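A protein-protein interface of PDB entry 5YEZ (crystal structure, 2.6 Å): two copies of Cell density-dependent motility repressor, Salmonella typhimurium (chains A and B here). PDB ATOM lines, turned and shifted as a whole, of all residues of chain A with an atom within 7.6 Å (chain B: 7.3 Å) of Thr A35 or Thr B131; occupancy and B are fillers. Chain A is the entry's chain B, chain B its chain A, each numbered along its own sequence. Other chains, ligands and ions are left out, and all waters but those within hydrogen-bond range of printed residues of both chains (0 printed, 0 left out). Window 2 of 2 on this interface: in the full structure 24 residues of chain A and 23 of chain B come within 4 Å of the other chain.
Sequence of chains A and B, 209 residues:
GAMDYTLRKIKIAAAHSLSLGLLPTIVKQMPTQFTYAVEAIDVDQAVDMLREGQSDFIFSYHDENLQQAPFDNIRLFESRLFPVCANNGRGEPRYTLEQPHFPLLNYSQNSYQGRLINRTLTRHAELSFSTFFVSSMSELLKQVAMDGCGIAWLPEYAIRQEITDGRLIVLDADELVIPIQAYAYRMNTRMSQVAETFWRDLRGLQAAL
The backbone NH of Val B134 sits at hydrogen-bond distance from the backbone carbonyl oxygen of Tyr A36 (2.9 Å).
The backbone NH (N) of Tyr A36 lies within hydrogen-bond range of the backbone carbonyl oxygen (O) of Phe B132 (2.9 Å).
The backbone carbonyl oxygen of Thr A35 sits at hydrogen-bond distance from the backbone NH of Ile A10, at 2.6 Å.
The backbone carbonyl oxygen (O) of Ile A10 sits at hydrogen-bond distance from the backbone NH (N) of Ala A37, at 3.2 Å.
The backbone NH (N) of Ile A12 sits at hydrogen-bond distance from the backbone carbonyl oxygen (O) of Ala A37, 2.9 Å away.
The backbone carbonyl oxygen (O) of Leu B104 is in hydrogen-bond range of the backbone NH (N) of Phe B132, 3.3 Å away.
The backbone carbonyl oxygen (O) of Arg A8 lies within hydrogen-bond range of the backbone NH (N) of Thr A35, 3.1 Å away.
The backbone carbonyl oxygen of Leu A7 is in hydrogen-bond range of the side-chain hydroxyl of Thr A35, 2.6 Å away.
Among the printed residues, merely in contact across the chains: Phe A34 with Phe B132 (3.1 Å), Ala A37 with Val B134 (3.3 Å), Thr A35 with Phe B132 (3.3 Å), Thr A35 with Thr B131 (3.3 Å) and Tyr A36 with Phe B133 (3.4 Å).
Lys A11 touches none of the printed residues of chain B.
Thr A32 touches none of the printed residues of chain B.
Of the printed residues of chain B, Phe A34 touches Phe B132.
Thr A35 touches two residues of chain B.
Of the printed residues of chain B, Tyr A36 touches Phe B132, Phe B133 and Val B134.
Of chain A, only Thr A35 (3.3 Å) comes within 4 Å of Thr B131.
Printed residues of chain A within 4 Å of Phe B132: Phe A34 (3.1 Å), Thr A35 (3.3 Å) and Tyr A36 (2.9 Å).
Of the printed residues of chain A, Phe B133 touches Tyr A36.
The nearest residue of chain A that does not touch Thr B131 is Leu A7 (5.3 Å).
The nearest printed residue of chain B that does not touch Ala A37 is Phe B133 (5.6 Å).
Of the 15 printed residues of chain B, 4 touch a printed residue of chain A.
Printed residues of chain A that touch a printed residue of chain B: Phe A34, Thr A35, Tyr A36 and Ala A37.
Hydrophobic or aromatic side chains of chain A that line the printed part of chain B: Tyr A36.
Among the printed residues, no Asp or Glu carboxylate lies within 4 Å of a Lys or Arg side-chain nitrogen of the other chain.
No position is printed for both chains.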
ATOM      1  N   LEU A   7     -35.245 -31.666 -19.996  1.00  0.00           N
ATOM      2  CA  LEU A   7     -35.968 -31.976 -18.769  1.00  0.00           C
ATOM      3  C   LEU A   7     -35.119 -31.671 -17.546  1.00  0.00           C
ATOM      4  O   LEU A   7     -33.888 -31.702 -17.598  1.00  0.00           O
ATOM      5  CB  LEU A   7     -36.406 -33.442 -18.750  1.00  0.00           C
ATOM      6  CG  LEU A   7     -35.449 -34.457 -18.120  1.00  0.00           C
ATOM      7  CD1 LEU A   7     -36.191 -35.741 -17.767  1.00  0.00           C
ATOM      8  CD2 LEU A   7     -34.279 -34.741 -19.047  1.00  0.00           C
ATOM      9  N   ARG A   8     -35.809 -31.409 -16.436  1.00  0.00           N
ATOM     10  CA  ARG A   8     -35.177 -30.955 -15.198  1.00  0.00           C
ATOM     11  C   ARG A   8     -34.266 -29.767 -15.487  1.00  0.00           C
ATOM     12  O   ARG A   8     -33.126 -29.683 -15.022  1.00  0.00           O
ATOM     13  CB  ARG A   8     -34.456 -32.113 -14.509  1.00  0.00           C
ATOM     14  CG  ARG A   8     -35.383 -33.313 -14.170  1.00  0.00           C
ATOM     15  CD  ARG A   8     -36.791 -32.907 -13.645  1.00  0.00           C
ATOM     16  NE  ARG A   8     -37.724 -32.453 -14.682  1.00  0.00           N
ATOM     17  CZ  ARG A   8     -38.406 -31.309 -14.641  1.00  0.00           C
ATOM     18  NH1 ARG A   8     -38.275 -30.477 -13.617  1.00  0.00           N
ATOM     19  NH2 ARG A   8     -39.214 -30.986 -15.640  1.00  0.00           N
ATOM     20  N   LYS A   9     -34.797 -28.846 -16.285  1.00  0.00           N
ATOM     21  CA  LYS A   9     -34.062 -27.680 -16.739  1.00  0.00           C
ATOM     22  C   LYS A   9     -33.872 -26.688 -15.603  1.00  0.00           C
ATOM     23  O   LYS A   9     -34.767 -26.476 -14.781  1.00  0.00           O
ATOM     24  CB  LYS A   9     -34.817 -27.020 -17.893  1.00  0.00           C
ATOM     25  CG  LYS A   9     -34.034 -26.882 -19.179  1.00  0.00           C
ATOM     26  CD  LYS A   9     -34.918 -26.297 -20.262  1.00  0.00           C
ATOM     27  CE  LYS A   9     -35.468 -24.948 -19.830  1.00  0.00           C
ATOM     28  NZ  LYS A   9     -36.020 -24.178 -20.975  1.00  0.00           N
ATOM     29  N   ILE A  10     -32.687 -26.095 -15.546  1.00  0.00           N
ATOM     30  CA  ILE A  10     -32.411 -24.983 -14.654  1.00  0.00           C
ATOM     31  C   ILE A  10     -32.060 -23.802 -15.548  1.00  0.00           C
ATOM     32  O   ILE A  10     -31.008 -23.797 -16.201  1.00  0.00           O
ATOM     33  CB  ILE A  10     -31.289 -25.307 -13.658  1.00  0.00           C
ATOM     34  CG1 ILE A  10     -31.830 -26.157 -12.501  1.00  0.00           C
ATOM     35  CG2 ILE A  10     -30.695 -24.037 -13.080  1.00  0.00           C
ATOM     36  CD1 ILE A  10     -32.940 -25.475 -11.706  1.00  0.00           C
ATOM     37  N   LYS A  11     -32.957 -22.823 -15.614  1.00  0.00           N
ATOM     38  CA  LYS A  11     -32.745 -21.631 -16.424  1.00  0.00           C
ATOM     39  C   LYS A  11     -32.019 -20.585 -15.593  1.00  0.00           C
ATOM     40  O   LYS A  11     -32.560 -20.084 -14.602  1.00  0.00           O
ATOM     41  CB  LYS A  11     -34.065 -21.073 -16.958  1.00  0.00           C
ATOM     42  CG  LYS A  11     -35.236 -22.036 -16.936  1.00  0.00           C
ATOM     43  CD  LYS A  11     -36.278 -21.640 -17.977  1.00  0.00           C
ATOM     44  CE  LYS A  11     -37.654 -22.188 -17.639  1.00  0.00           C
ATOM     45  NZ  LYS A  11     -38.348 -21.304 -16.661  1.00  0.00           N
ATOM     46  N   ILE A  12     -30.795 -20.261 -15.997  1.00  0.00           N
ATOM     47  CA  ILE A  12     -29.984 -19.248 -15.339  1.00  0.00           C
ATOM     48  C   ILE A  12     -29.719 -18.135 -16.339  1.00  0.00           C
ATOM     49  O   ILE A  12     -29.400 -18.402 -17.504  1.00  0.00           O
ATOM     50  CB  ILE A  12     -28.659 -19.826 -14.807  1.00  0.00           C
ATOM     51  CG1 ILE A  12     -28.841 -21.285 -14.386  1.00  0.00           C
ATOM     52  CG2 ILE A  12     -28.144 -18.993 -13.643  1.00  0.00           C
ATOM     53  CD1 ILE A  12     -27.613 -21.894 -13.747  1.00  0.00           C
ATOM     54  N   THR A  32     -25.736 -33.791  -8.369  1.00  0.00           N
ATOM     55  CA  THR A  32     -26.649 -34.463  -9.279  1.00  0.00           C
ATOM     56  C   THR A  32     -26.673 -33.741 -10.622  1.00  0.00           C
ATOM     57  O   THR A  32     -26.149 -32.634 -10.773  1.00  0.00           O
ATOM     58  CB  THR A  32     -28.059 -34.551  -8.681  1.00  0.00           C
ATOM     59  OG1 THR A  32     -28.994 -34.924  -9.701  1.00  0.00           O
ATOM     60  CG2 THR A  32     -28.466 -33.223  -8.069  1.00  0.00           C
ATOM     61  N   GLN A  33     -27.292 -34.388 -11.606  1.00  0.00           N
ATOM     62  CA  GLN A  33     -27.233 -33.954 -12.996  1.00  0.00           C
ATOM     63  C   GLN A  33     -28.538 -33.280 -13.395  1.00  0.00           C
ATOM     64  O   GLN A  33     -29.618 -33.857 -13.226  1.00  0.00           O
ATOM     65  CB  GLN A  33     -26.942 -35.140 -13.919  1.00  0.00           C
ATOM     66  CG  GLN A  33     -25.462 -35.372 -14.186  1.00  0.00           C
ATOM     67  CD  GLN A  33     -24.593 -35.054 -12.983  1.00  0.00           C
ATOM     68  OE1 GLN A  33     -23.904 -34.034 -12.952  1.00  0.00           O
ATOM     69  NE2 GLN A  33     -24.625 -35.927 -11.983  1.00  0.00           N
ATOM     70  N   PHE A  34     -28.433 -32.067 -13.930  1.00  0.00           N
ATOM     71  CA  PHE A  34     -29.571 -31.281 -14.391  1.00  0.00           C
ATOM     72  C   PHE A  34     -29.446 -31.013 -15.891  1.00  0.00           C
ATOM     73  O   PHE A  34     -28.579 -31.560 -16.578  1.00  0.00           O
ATOM     74  CB  PHE A  34     -29.671 -29.955 -13.632  1.00  0.00           C
ATOM     75  CG  PHE A  34     -29.587 -30.085 -12.140  1.00  0.00           C
ATOM     76  CD1 PHE A  34     -30.728 -30.286 -11.388  1.00  0.00           C
ATOM     77  CD2 PHE A  34     -28.370 -29.975 -11.486  1.00  0.00           C
ATOM     78  CE1 PHE A  34     -30.663 -30.393 -10.015  1.00  0.00           C
ATOM     79  CE2 PHE A  34     -28.297 -30.081 -10.111  1.00  0.00           C
ATOM     80  CZ  PHE A  34     -29.447 -30.288  -9.374  1.00  0.00           C
ATOM     81  N   THR A  35     -30.334 -30.156 -16.390  1.00  0.00           N
ATOM     82  CA  THR A  35     -30.227 -29.550 -17.709  1.00  0.00           C
ATOM     83  C   THR A  35     -30.145 -28.041 -17.526  1.00  0.00           C
ATOM     84  O   THR A  35     -30.839 -27.476 -16.674  1.00  0.00           O
ATOM     85  CB  THR A  35     -31.424 -29.915 -18.598  1.00  0.00           C
ATOM     86  OG1 THR A  35     -31.516 -31.339 -18.721  1.00  0.00           O
ATOM     87  CG2 THR A  35     -31.275 -29.302 -19.984  1.00  0.00           C
ATOM     88  N   TYR A  36     -29.292 -27.387 -18.310  1.00  0.00           N
ATOM     89  CA  TYR A  36     -28.999 -25.974 -18.120  1.00  0.00           C
ATOM     90  C   TYR A  36     -29.338 -25.176 -19.370  1.00  0.00           C
ATOM     91  O   TYR A  36     -29.114 -25.634 -20.495  1.00  0.00           O
ATOM     92  CB  TYR A  36     -27.525 -25.762 -17.765  1.00  0.00           C
ATOM     93  CG  TYR A  36     -27.094 -26.421 -16.475  1.00  0.00           C
ATOM     94  CD1 TYR A  36     -26.761 -27.770 -16.439  1.00  0.00           C
ATOM     95  CD2 TYR A  36     -27.006 -25.693 -15.297  1.00  0.00           C
ATOM     96  CE1 TYR A  36     -26.364 -28.374 -15.266  1.00  0.00           C
ATOM     97  CE2 TYR A  36     -26.607 -26.289 -14.117  1.00  0.00           C
ATOM     98  CZ  TYR A  36     -26.288 -27.630 -14.107  1.00  0.00           C
ATOM     99  OH  TYR A  36     -25.891 -28.232 -12.936  1.00  0.00           O
ATOM    100  N   ALA A  37     -29.876 -23.976 -19.160  1.00  0.00           N
ATOM    101  CA  ALA A  37     -30.113 -22.997 -20.218  1.00  0.00           C
ATOM    102  C   ALA A  37     -29.612 -21.654 -19.704  1.00  0.00           C
ATOM    103  O   ALA A  37     -30.161 -21.116 -18.737  1.00  0.00           O
ATOM    104  CB  ALA A  37     -31.593 -22.928 -20.596  1.00  0.00           C
ATOM    105  N   ASP A  56     -34.977 -19.129 -13.319  1.00  0.00           N
ATOM    106  CA  ASP A  56     -35.111 -19.578 -11.940  1.00  0.00           C
ATOM    107  C   ASP A  56     -34.048 -18.968 -11.038  1.00  0.00           C
ATOM    108  O   ASP A  56     -34.310 -18.723  -9.856  1.00  0.00           O
ATOM    109  CB  ASP A  56     -35.045 -21.104 -11.880  1.00  0.00           C
ATOM    110  CG  ASP A  56     -36.008 -21.765 -12.846  1.00  0.00           C
ATOM    111  OD1 ASP A  56     -37.061 -21.161 -13.144  1.00  0.00           O
ATOM    112  OD2 ASP A  56     -35.709 -22.885 -13.315  1.00  0.00           O
ATOM    113  N   VAL A 194     -36.752 -29.328  -8.602  1.00  0.00           N
ATOM    114  CA  VAL A 194     -35.391 -29.374  -9.120  1.00  0.00           C
ATOM    115  C   VAL A 194     -34.639 -28.098  -8.779  1.00  0.00           C
ATOM    116  O   VAL A 194     -33.433 -28.129  -8.513  1.00  0.00           O
ATOM    117  CB  VAL A 194     -35.428 -29.632 -10.636  1.00  0.00           C
ATOM    118  CG1 VAL A 194     -34.101 -30.168 -11.113  1.00  0.00           C
ATOM    119  CG2 VAL A 194     -36.536 -30.609 -10.958  1.00  0.00           C
ATOM    120  N   PHE A 198     -31.168 -27.825  -6.900  1.00  0.00           N
ATOM    121  CA  PHE A 198     -30.001 -27.128  -7.431  1.00  0.00           C
ATOM    122  C   PHE A 198     -29.526 -26.039  -6.476  1.00  0.00           C
ATOM    123  O   PHE A 198     -28.319 -25.875  -6.263  1.00  0.00           O
ATOM    124  CB  PHE A 198     -30.326 -26.538  -8.804  1.00  0.00           C
ATOM    125  CG  PHE A 198     -29.293 -25.572  -9.316  1.00  0.00           C
ATOM    126  CD1 PHE A 198     -29.440 -24.207  -9.122  1.00  0.00           C
ATOM    127  CD2 PHE A 198     -28.178 -26.029  -9.999  1.00  0.00           C
ATOM    128  CE1 PHE A 198     -28.492 -23.319  -9.593  1.00  0.00           C
ATOM    129  CE2 PHE A 198     -27.227 -25.144 -10.473  1.00  0.00           C
ATOM    130  CZ  PHE A 198     -27.385 -23.787 -10.270  1.00  0.00           C
ATOM    131  N   PHE B 102     -25.956 -39.453 -25.469  1.00  0.00           N
ATOM    132  CA  PHE B 102     -24.804 -38.706 -24.984  1.00  0.00           C
ATOM    133  C   PHE B 102     -25.215 -37.272 -24.650  1.00  0.00           C
ATOM    134  O   PHE B 102     -26.081 -36.702 -25.320  1.00  0.00           O
ATOM    135  CB  PHE B 102     -23.671 -38.708 -26.016  1.00  0.00           C
ATOM    136  CG  PHE B 102     -24.023 -38.056 -27.328  1.00  0.00           C
ATOM    137  CD1 PHE B 102     -23.890 -36.685 -27.501  1.00  0.00           C
ATOM    138  CD2 PHE B 102     -24.458 -38.819 -28.399  1.00  0.00           C
ATOM    139  CE1 PHE B 102     -24.201 -36.088 -28.708  1.00  0.00           C
ATOM    140  CE2 PHE B 102     -24.772 -38.227 -29.610  1.00  0.00           C
ATOM    141  CZ  PHE B 102     -24.640 -36.860 -29.764  1.00  0.00           C
ATOM    142  N   PRO B 103     -24.628 -36.675 -23.613  1.00  0.00           N
ATOM    143  CA  PRO B 103     -24.966 -35.286 -23.275  1.00  0.00           C
ATOM    144  C   PRO B 103     -24.482 -34.335 -24.360  1.00  0.00           C
ATOM    145  O   PRO B 103     -23.316 -34.368 -24.759  1.00  0.00           O
ATOM    146  CB  PRO B 103     -24.236 -35.052 -21.947  1.00  0.00           C
ATOM    147  CG  PRO B 103     -23.132 -36.060 -21.941  1.00  0.00           C
ATOM    148  CD  PRO B 103     -23.657 -37.258 -22.672  1.00  0.00           C
ATOM    149  N   LEU B 104     -25.391 -33.491 -24.841  1.00  0.00           N
ATOM    150  CA  LEU B 104     -25.122 -32.590 -25.957  1.00  0.00           C
ATOM    151  C   LEU B 104     -25.044 -31.159 -25.441  1.00  0.00           C
ATOM    152  O   LEU B 104     -26.040 -30.612 -24.955  1.00  0.00           O
ATOM    153  CB  LEU B 104     -26.196 -32.720 -27.034  1.00  0.00           C
ATOM    154  CG  LEU B 104     -26.148 -31.658 -28.135  1.00  0.00           C
ATOM    155  CD1 LEU B 104     -25.082 -31.998 -29.167  1.00  0.00           C
ATOM    156  CD2 LEU B 104     -27.509 -31.497 -28.797  1.00  0.00           C
ATOM    157  N   LEU B 105     -23.863 -30.558 -25.548  1.00  0.00           N
ATOM    158  CA  LEU B 105     -23.696 -29.128 -25.324  1.00  0.00           C
ATOM    159  C   LEU B 105     -23.895 -28.418 -26.656  1.00  0.00           C
ATOM    160  O   LEU B 105     -23.140 -28.651 -27.607  1.00  0.00           O
ATOM    161  CB  LEU B 105     -22.315 -28.823 -24.746  1.00  0.00           C
ATOM    162  CG  LEU B 105     -21.731 -29.877 -23.808  1.00  0.00           C
ATOM    163  CD1 LEU B 105     -20.235 -29.680 -23.664  1.00  0.00           C
ATOM    164  CD2 LEU B 105     -22.410 -29.819 -22.453  1.00  0.00           C
ATOM    165  N   ASN B 106     -24.912 -27.564 -26.731  1.00  0.00           N
ATOM    166  CA  ASN B 106     -25.279 -26.962 -28.003  1.00  0.00           C
ATOM    167  C   ASN B 106     -25.778 -25.545 -27.770  1.00  0.00           C
ATOM    168  O   ASN B 106     -26.199 -25.184 -26.668  1.00  0.00           O
ATOM    169  CB  ASN B 106     -26.346 -27.796 -28.724  1.00  0.00           C
ATOM    170  CG  ASN B 106     -26.648 -27.283 -30.119  1.00  0.00           C
ATOM    171  OD1 ASN B 106     -25.977 -26.380 -30.623  1.00  0.00           O
ATOM    172  ND2 ASN B 106     -27.665 -27.856 -30.752  1.00  0.00           N
ATOM    173  N   TYR B 107     -25.719 -24.742 -28.828  1.00  0.00           N
ATOM    174  CA  TYR B 107     -26.307 -23.416 -28.807  1.00  0.00           C
ATOM    175  C   TYR B 107     -27.830 -23.517 -28.752  1.00  0.00           C
ATOM    176  O   TYR B 107     -28.421 -24.587 -28.924  1.00  0.00           O
ATOM    177  CB  TYR B 107     -25.889 -22.616 -30.041  1.00  0.00           C
ATOM    178  CG  TYR B 107     -24.422 -22.711 -30.400  1.00  0.00           C
ATOM    179  CD1 TYR B 107     -23.933 -23.786 -31.133  1.00  0.00           C
ATOM    180  CD2 TYR B 107     -23.530 -21.714 -30.026  1.00  0.00           C
ATOM    181  CE1 TYR B 107     -22.596 -23.872 -31.467  1.00  0.00           C
ATOM    182  CE2 TYR B 107     -22.192 -21.791 -30.358  1.00  0.00           C
ATOM    183  CZ  TYR B 107     -21.730 -22.873 -31.079  1.00  0.00           C
ATOM    184  OH  TYR B 107     -20.399 -22.956 -31.413  1.00  0.00           O
ATOM    185  N   GLN B 109     -31.669 -22.238 -30.253  1.00  0.00           N
ATOM    186  CA  GLN B 109     -32.229 -21.965 -31.569  1.00  0.00           C
ATOM    187  C   GLN B 109     -32.191 -20.483 -31.912  1.00  0.00           C
ATOM    188  O   GLN B 109     -32.461 -20.120 -33.061  1.00  0.00           O
ATOM    189  CB  GLN B 109     -33.663 -22.490 -31.651  1.00  0.00           C
ATOM    190  CG  GLN B 109     -33.785 -23.999 -31.472  1.00  0.00           C
ATOM    191  CD  GLN B 109     -33.758 -24.426 -30.014  1.00  0.00           C
ATOM    192  OE1 GLN B 109     -33.577 -23.602 -29.116  1.00  0.00           O
ATOM    193  NE2 GLN B 109     -33.940 -25.719 -29.772  1.00  0.00           N
ATOM    194  N   ASN B 118     -28.771 -28.770 -34.978  1.00  0.00           N
ATOM    195  CA  ASN B 118     -29.991 -29.546 -34.781  1.00  0.00           C
ATOM    196  C   ASN B 118     -30.511 -30.128 -36.090  1.00  0.00           C
ATOM    197  O   ASN B 118     -31.082 -31.224 -36.094  1.00  0.00           O
ATOM    198  CB  ASN B 118     -31.063 -28.679 -34.121  1.00  0.00           C
ATOM    199  CG  ASN B 118     -30.984 -28.706 -32.607  1.00  0.00           C
ATOM    200  OD1 ASN B 118     -29.915 -28.912 -32.034  1.00  0.00           O
ATOM    201  ND2 ASN B 118     -32.120 -28.499 -31.952  1.00  0.00           N
ATOM    202  N   LEU B 121     -28.290 -33.191 -36.886  1.00  0.00           N
ATOM    203  CA  LEU B 121     -28.773 -34.339 -36.129  1.00  0.00           C
ATOM    204  C   LEU B 121     -30.149 -34.797 -36.597  1.00  0.00           C
ATOM    205  O   LEU B 121     -30.541 -35.932 -36.308  1.00  0.00           O
ATOM    206  CB  LEU B 121     -28.816 -34.011 -34.635  1.00  0.00           C
ATOM    207  CG  LEU B 121     -27.568 -33.371 -34.024  1.00  0.00           C
ATOM    208  CD1 LEU B 121     -27.690 -33.295 -32.510  1.00  0.00           C
ATOM    209  CD2 LEU B 121     -26.307 -34.125 -34.426  1.00  0.00           C
ATOM    210  N   PHE B 129     -28.973 -38.557 -28.488  1.00  0.00           N
ATOM    211  CA  PHE B 129     -28.333 -37.562 -27.642  1.00  0.00           C
ATOM    212  C   PHE B 129     -29.318 -37.065 -26.593  1.00  0.00           C
ATOM    213  O   PHE B 129     -30.524 -37.316 -26.665  1.00  0.00           O
ATOM    214  CB  PHE B 129     -27.796 -36.384 -28.467  1.00  0.00           C
ATOM    215  CG  PHE B 129     -28.859 -35.633 -29.219  1.00  0.00           C
ATOM    216  CD1 PHE B 129     -29.280 -36.063 -30.466  1.00  0.00           C
ATOM    217  CD2 PHE B 129     -29.429 -34.491 -28.682  1.00  0.00           C
ATOM    218  CE1 PHE B 129     -30.257 -35.373 -31.160  1.00  0.00           C
ATOM    219  CE2 PHE B 129     -30.406 -33.795 -29.372  1.00  0.00           C
ATOM    220  CZ  PHE B 129     -30.821 -34.236 -30.612  1.00  0.00           C
ATOM    221  N   SER B 130     -28.782 -36.347 -25.610  1.00  0.00           N
ATOM    222  CA  SER B 130     -29.574 -35.743 -24.548  1.00  0.00           C
ATOM    223  C   SER B 130     -29.160 -34.287 -24.411  1.00  0.00           C
ATOM    224  O   SER B 130     -28.007 -33.999 -24.077  1.00  0.00           O
ATOM    225  CB  SER B 130     -29.382 -36.485 -23.223  1.00  0.00           C
ATOM    226  OG  SER B 130     -29.952 -37.780 -23.278  1.00  0.00           O
ATOM    227  N   THR B 131     -30.094 -33.376 -24.681  1.00  0.00           N
ATOM    228  CA  THR B 131     -29.833 -31.951 -24.516  1.00  0.00           C
ATOM    229  C   THR B 131     -29.549 -31.643 -23.051  1.00  0.00           C
ATOM    230  O   THR B 131     -30.461 -31.650 -22.218  1.00  0.00           O
ATOM    231  CB  THR B 131     -31.014 -31.122 -25.027  1.00  0.00           C
ATOM    232  OG1 THR B 131     -31.165 -31.325 -26.437  1.00  0.00           O
ATOM    233  CG2 THR B 131     -30.785 -29.646 -24.757  1.00  0.00           C
ATOM    234  N   PHE B 132     -28.284 -31.381 -22.731  1.00  0.00           N
ATOM    235  CA  PHE B 132     -27.833 -31.201 -21.356  1.00  0.00           C
ATOM    236  C   PHE B 132     -27.507 -29.759 -21.004  1.00  0.00           C
ATOM    237  O   PHE B 132     -27.831 -29.312 -19.902  1.00  0.00           O
ATOM    238  CB  PHE B 132     -26.605 -32.083 -21.097  1.00  0.00           C
ATOM    239  CG  PHE B 132     -25.795 -31.666 -19.904  1.00  0.00           C
ATOM    240  CD1 PHE B 132     -26.274 -31.864 -18.622  1.00  0.00           C
ATOM    241  CD2 PHE B 132     -24.548 -31.087 -20.066  1.00  0.00           C
ATOM    242  CE1 PHE B 132     -25.528 -31.484 -17.522  1.00  0.00           C
ATOM    243  CE2 PHE B 132     -23.797 -30.704 -18.973  1.00  0.00           C
ATOM    244  CZ  PHE B 132     -24.287 -30.903 -17.699  1.00  0.00           C
ATOM    245  N   PHE B 133     -26.882 -29.013 -21.912  1.00  0.00           N
ATOM    246  CA  PHE B 133     -26.494 -27.630 -21.655  1.00  0.00           C
ATOM    247  C   PHE B 133     -26.690 -26.835 -22.935  1.00  0.00           C
ATOM    248  O   PHE B 133     -26.121 -27.185 -23.973  1.00  0.00           O
ATOM    249  CB  PHE B 133     -25.038 -27.547 -21.174  1.00  0.00           C
ATOM    250  CG  PHE B 133     -24.594 -26.159 -20.788  1.00  0.00           C
ATOM    251  CD1 PHE B 133     -24.204 -25.244 -21.753  1.00  0.00           C
ATOM    252  CD2 PHE B 133     -24.550 -25.777 -19.457  1.00  0.00           C
ATOM    253  CE1 PHE B 133     -23.795 -23.973 -21.401  1.00  0.00           C
ATOM    254  CE2 PHE B 133     -24.140 -24.506 -19.097  1.00  0.00           C
ATOM    255  CZ  PHE B 133     -23.758 -23.605 -20.071  1.00  0.00           C
ATOM    256  N   VAL B 134     -27.487 -25.769 -22.865  1.00  0.00           N
ATOM    257  CA  VAL B 134     -27.790 -24.939 -24.024  1.00  0.00           C
ATOM    258  C   VAL B 134     -27.481 -23.489 -23.679  1.00  0.00           C
ATOM    259  O   VAL B 134     -28.005 -22.956 -22.693  1.00  0.00           O
ATOM    260  CB  VAL B 134     -29.252 -25.092 -24.480  1.00  0.00           C
ATOM    261  CG1 VAL B 134     -29.704 -23.867 -25.264  1.00  0.00           C
ATOM    262  CG2 VAL B 134     -29.409 -26.346 -25.323  1.00  0.00           C
